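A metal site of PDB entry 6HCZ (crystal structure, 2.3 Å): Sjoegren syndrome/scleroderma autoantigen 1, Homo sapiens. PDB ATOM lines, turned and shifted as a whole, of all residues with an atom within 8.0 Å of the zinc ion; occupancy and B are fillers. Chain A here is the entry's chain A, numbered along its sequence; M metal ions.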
ATOM      1  N   ARG A  30       2.542 -11.652   8.558  1.00  0.00           N
ATOM      2  CA  ARG A  30       1.926 -12.678   9.397  1.00  0.00           C
ATOM      3  C   ARG A  30       0.924 -12.010  10.343  1.00  0.00           C
ATOM      4  O   ARG A  30      -0.244 -12.364  10.414  1.00  0.00           O
ATOM      5  CB  ARG A  30       2.981 -13.430  10.186  1.00  0.00           C
ATOM      6  CG  ARG A  30       2.555 -14.795  10.698  1.00  0.00           C
ATOM      7  CD  ARG A  30       3.355 -15.254  11.919  1.00  0.00           C
ATOM      8  NE  ARG A  30       3.001 -16.621  12.255  1.00  0.00           N
ATOM      9  CZ  ARG A  30       2.552 -17.082  13.429  1.00  0.00           C
ATOM     10  NH1 ARG A  30       2.766 -16.383  14.541  1.00  0.00           N
ATOM     11  NH2 ARG A  30       1.924 -18.252  13.470  1.00  0.00           N
ATOM     12  N   ILE A  34      -2.982 -12.524  10.674  1.00  0.00           N
ATOM     13  CA  ILE A  34      -3.608 -13.047  11.908  1.00  0.00           C
ATOM     14  C   ILE A  34      -4.776 -12.132  12.294  1.00  0.00           C
ATOM     15  O   ILE A  34      -5.905 -12.603  12.603  1.00  0.00           O
ATOM     16  CB  ILE A  34      -2.580 -13.195  13.058  1.00  0.00           C
ATOM     17  CG1 ILE A  34      -1.590 -14.330  12.799  1.00  0.00           C
ATOM     18  CG2 ILE A  34      -3.243 -13.381  14.418  1.00  0.00           C
ATOM     19  CD1 ILE A  34      -0.314 -14.209  13.627  1.00  0.00           C
ATOM     20  N   THR A  52      -4.397 -16.987  25.306  1.00  0.00           N
ATOM     21  CA  THR A  52      -3.482 -17.005  24.193  1.00  0.00           C
ATOM     22  C   THR A  52      -2.919 -18.408  23.960  1.00  0.00           C
ATOM     23  O   THR A  52      -2.678 -19.223  24.844  1.00  0.00           O
ATOM     24  CB  THR A  52      -2.336 -16.000  24.411  1.00  0.00           C
ATOM     25  OG1 THR A  52      -1.617 -16.389  25.582  1.00  0.00           O
ATOM     26  CG2 THR A  52      -2.822 -14.577  24.552  1.00  0.00           C
ATOM     27  N   CYS A  53      -2.718 -18.683  22.680  1.00  0.00           N
ATOM     28  CA  CYS A  53      -2.165 -19.902  22.213  1.00  0.00           C
ATOM     29  C   CYS A  53      -0.823 -20.122  22.916  1.00  0.00           C
ATOM     30  O   CYS A  53      -0.006 -19.224  22.959  1.00  0.00           O
ATOM     31  CB  CYS A  53      -2.001 -19.801  20.707  1.00  0.00           C
ATOM     32  SG  CYS A  53      -1.259 -21.288  20.039  1.00  0.00           S
ATOM     33  N   ALA A  54      -0.640 -21.311  23.475  1.00  0.00           N
ATOM     34  CA  ALA A  54       0.534 -21.647  24.297  1.00  0.00           C
ATOM     35  C   ALA A  54       1.765 -21.814  23.413  1.00  0.00           C
ATOM     36  O   ALA A  54       2.856 -21.501  23.838  1.00  0.00           O
ATOM     37  CB  ALA A  54       0.257 -22.869  25.138  1.00  0.00           C
ATOM     38  N   ASP A  55       1.572 -22.305  22.177  1.00  0.00           N
ATOM     39  CA  ASP A  55       2.647 -22.397  21.148  1.00  0.00           C
ATOM     40  C   ASP A  55       3.073 -20.997  20.661  1.00  0.00           C
ATOM     41  O   ASP A  55       4.252 -20.731  20.595  1.00  0.00           O
ATOM     42  CB  ASP A  55       2.224 -23.272  19.963  1.00  0.00           C
ATOM     43  CG  ASP A  55       2.044 -24.737  20.291  1.00  0.00           C
ATOM     44  OD1 ASP A  55       2.962 -25.331  20.886  1.00  0.00           O
ATOM     45  OD2 ASP A  55       0.976 -25.288  19.977  1.00  0.00           O
ATOM     46  N   CYS A  56       2.131 -20.108  20.325  1.00  0.00           N
ATOM     47  CA  CYS A  56       2.453 -18.933  19.465  1.00  0.00           C
ATOM     48  C   CYS A  56       2.017 -17.563  20.036  1.00  0.00           C
ATOM     49  O   CYS A  56       2.399 -16.568  19.491  1.00  0.00           O
ATOM     50  CB  CYS A  56       1.847 -19.116  18.081  1.00  0.00           C
ATOM     51  SG  CYS A  56       0.099 -18.671  17.978  1.00  0.00           S
ATOM     52  N   GLY A  57       1.195 -17.501  21.093  1.00  0.00           N
ATOM     53  CA  GLY A  57       0.892 -16.224  21.749  1.00  0.00           C
ATOM     54  C   GLY A  57      -0.401 -15.567  21.275  1.00  0.00           C
ATOM     55  O   GLY A  57      -0.916 -14.661  21.932  1.00  0.00           O
ATOM     56  N   THR A  58      -0.939 -15.996  20.132  1.00  0.00           N
ATOM     57  CA  THR A  58      -2.155 -15.432  19.546  1.00  0.00           C
ATOM     58  C   THR A  58      -3.398 -15.681  20.427  1.00  0.00           C
ATOM     59  O   THR A  58      -3.603 -16.783  20.923  1.00  0.00           O
ATOM     60  CB  THR A  58      -2.412 -16.070  18.179  1.00  0.00           C
ATOM     61  OG1 THR A  58      -1.211 -15.940  17.438  1.00  0.00           O
ATOM     62  CG2 THR A  58      -3.567 -15.463  17.425  1.00  0.00           C
ATOM     63  N   ILE A  59      -4.279 -14.679  20.521  1.00  0.00           N
ATOM     64  CA  ILE A  59      -5.567 -14.858  21.188  1.00  0.00           C
ATOM     65  C   ILE A  59      -6.318 -15.998  20.490  1.00  0.00           C
ATOM     66  O   ILE A  59      -6.257 -16.138  19.279  1.00  0.00           O
ATOM     67  CB  ILE A  59      -6.402 -13.575  21.184  1.00  0.00           C
ATOM     68  CG1 ILE A  59      -5.977 -12.629  22.295  1.00  0.00           C
ATOM     69  CG2 ILE A  59      -7.879 -13.904  21.282  1.00  0.00           C
ATOM     70  CD1 ILE A  59      -6.187 -11.173  21.964  1.00  0.00           C
ATOM     71  N   LEU A  60      -7.018 -16.795  21.288  1.00  0.00           N
ATOM     72  CA  LEU A  60      -7.707 -17.982  20.839  1.00  0.00           C
ATOM     73  C   LEU A  60      -9.185 -17.654  20.632  1.00  0.00           C
ATOM     74  O   LEU A  60      -9.738 -16.690  21.228  1.00  0.00           O
ATOM     75  CB  LEU A  60      -7.529 -19.098  21.878  1.00  0.00           C
ATOM     76  CG  LEU A  60      -6.123 -19.702  22.027  1.00  0.00           C
ATOM     77  CD1 LEU A  60      -6.054 -20.713  23.170  1.00  0.00           C
ATOM     78  CD2 LEU A  60      -5.662 -20.339  20.725  1.00  0.00           C
ATOM     79  N   TYR A  69      -9.495 -22.786  18.884  1.00  0.00           N
ATOM     80  CA  TYR A  69      -9.019 -22.510  17.542  1.00  0.00           C
ATOM     81  C   TYR A  69      -8.024 -21.347  17.568  1.00  0.00           C
ATOM     82  O   TYR A  69      -8.387 -20.207  17.999  1.00  0.00           O
ATOM     83  CB  TYR A  69     -10.227 -22.192  16.634  1.00  0.00           C
ATOM     84  CG  TYR A  69      -9.881 -22.149  15.177  1.00  0.00           C
ATOM     85  CD1 TYR A  69      -9.837 -23.312  14.434  1.00  0.00           C
ATOM     86  CD2 TYR A  69      -9.521 -20.959  14.551  1.00  0.00           C
ATOM     87  CE1 TYR A  69      -9.469 -23.294  13.095  1.00  0.00           C
ATOM     88  CE2 TYR A  69      -9.147 -20.919  13.220  1.00  0.00           C
ATOM     89  CZ  TYR A  69      -9.126 -22.099  12.495  1.00  0.00           C
ATOM     90  OH  TYR A  69      -8.782 -22.099  11.174  1.00  0.00           O
ATOM     91  N   CYS A  70      -6.778 -21.629  17.163  1.00  0.00           N
ATOM     92  CA  CYS A  70      -5.723 -20.636  16.967  1.00  0.00           C
ATOM     93  C   CYS A  70      -5.530 -20.398  15.467  1.00  0.00           C
ATOM     94  O   CYS A  70      -5.037 -21.312  14.763  1.00  0.00           O
ATOM     95  CB  CYS A  70      -4.384 -21.072  17.552  1.00  0.00           C
ATOM     96  SG  CYS A  70      -3.006 -19.963  17.131  1.00  0.00           S
ATOM     97  N   VAL A  71      -5.858 -19.166  15.014  1.00  0.00           N
ATOM     98  CA  VAL A  71      -5.834 -18.779  13.592  1.00  0.00           C
ATOM     99  C   VAL A  71      -4.399 -18.886  13.052  1.00  0.00           C
ATOM    100  O   VAL A  71      -4.179 -19.250  11.910  1.00  0.00           O
ATOM    101  CB  VAL A  71      -6.427 -17.371  13.351  1.00  0.00           C
ATOM    102  CG1 VAL A  71      -7.918 -17.328  13.608  1.00  0.00           C
ATOM    103  CG2 VAL A  71      -5.734 -16.299  14.173  1.00  0.00           C
ATOM    104  N   ALA A  72      -3.417 -18.569  13.893  1.00  0.00           N
ATOM    105  CA  ALA A  72      -2.044 -18.659  13.467  1.00  0.00           C
ATOM    106  C   ALA A  72      -1.711 -20.136  13.280  1.00  0.00           C
ATOM    107  O   ALA A  72      -1.348 -20.587  12.199  1.00  0.00           O
ATOM    108  CB  ALA A  72      -1.122 -18.004  14.473  1.00  0.00           C
ATOM    109  N   CYS A  73      -1.883 -20.904  14.351  1.00  0.00           N
ATOM    110  CA  CYS A  73      -1.403 -22.268  14.339  1.00  0.00           C
ATOM    111  C   CYS A  73      -2.222 -23.110  13.352  1.00  0.00           C
ATOM    112  O   CYS A  73      -1.638 -23.841  12.580  1.00  0.00           O
ATOM    113  CB  CYS A  73      -1.414 -22.874  15.741  1.00  0.00           C
ATOM    114  SG  CYS A  73       0.029 -22.342  16.718  1.00  0.00           S
ATOM    115  N   GLN A  74      -3.551 -22.967  13.353  1.00  0.00           N
ATOM    116  CA  GLN A  74      -4.410 -23.871  12.599  1.00  0.00           C
ATOM    117  C   GLN A  74      -4.831 -23.234  11.266  1.00  0.00           C
ATOM    118  O   GLN A  74      -5.807 -23.657  10.685  1.00  0.00           O
ATOM    119  CB  GLN A  74      -5.637 -24.285  13.429  1.00  0.00           C
ATOM    120  CG  GLN A  74      -5.396 -25.533  14.287  1.00  0.00           C
ATOM    121  CD  GLN A  74      -6.324 -25.620  15.469  1.00  0.00           C
ATOM    122  OE1 GLN A  74      -7.063 -26.588  15.630  1.00  0.00           O
ATOM    123  NE2 GLN A  74      -6.282 -24.603  16.330  1.00  0.00           N
ATOM    124  N   GLU A  75      -4.070 -22.254  10.776  1.00  0.00           N
ATOM    125  CA  GLU A  75      -4.288 -21.722   9.420  1.00  0.00           C
ATOM    126  C   GLU A  75      -3.047 -21.019   8.862  1.00  0.00           C
ATOM    127  O   GLU A  75      -3.140 -20.424   7.813  1.00  0.00           O
ATOM    128  CB  GLU A  75      -5.502 -20.794   9.422  1.00  0.00           C
ATOM    129  CG  GLU A  75      -6.381 -20.933   8.199  1.00  0.00           C
ATOM    130  CD  GLU A  75      -7.783 -20.357   8.306  1.00  0.00           C
ATOM    131  OE1 GLU A  75      -8.334 -19.946   7.248  1.00  0.00           O
ATOM    132  OE2 GLU A  75      -8.330 -20.327   9.431  1.00  0.00           O
HETATM  133 ZN    ZN M   1      -1.113 -20.706  17.929  1.00  0.00          ZN
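The side-chain sulfur (SG) of Cys 70 sits close to the backbone NH (N) of Ala 72 (3.5 Å).
NE2 of Gln 74 sits close to N of Cys 70.
SG of Cys 53 lies close to N of Asp 55.
O of Thr 58 sits at hydrogen-bond distance from N of Cys 53 (2.7 Å).
The side-chain sulfur (SG) of Cys 56 sits close to the side-chain hydroxyl (OG1) of Thr 58.
Four residues have an atom within 4 Å of the zinc ion: Cys 53, Cys 56, Cys 70 and Cys 73.
The nearest printed residue that does not touch the zinc ion is Ala 72 (4.4 Å).
The zinc ion is bound by the side-chain sulfur of Cys 70 (2.2 Å), the side-chain sulfur of Cys 53 (2.2 Å), the side-chain sulfur of Cys 73 (2.3 Å) and the side-chain sulfur of Cys 56 (2.4 Å).
The zinc ion has four donor atoms within binding distance.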
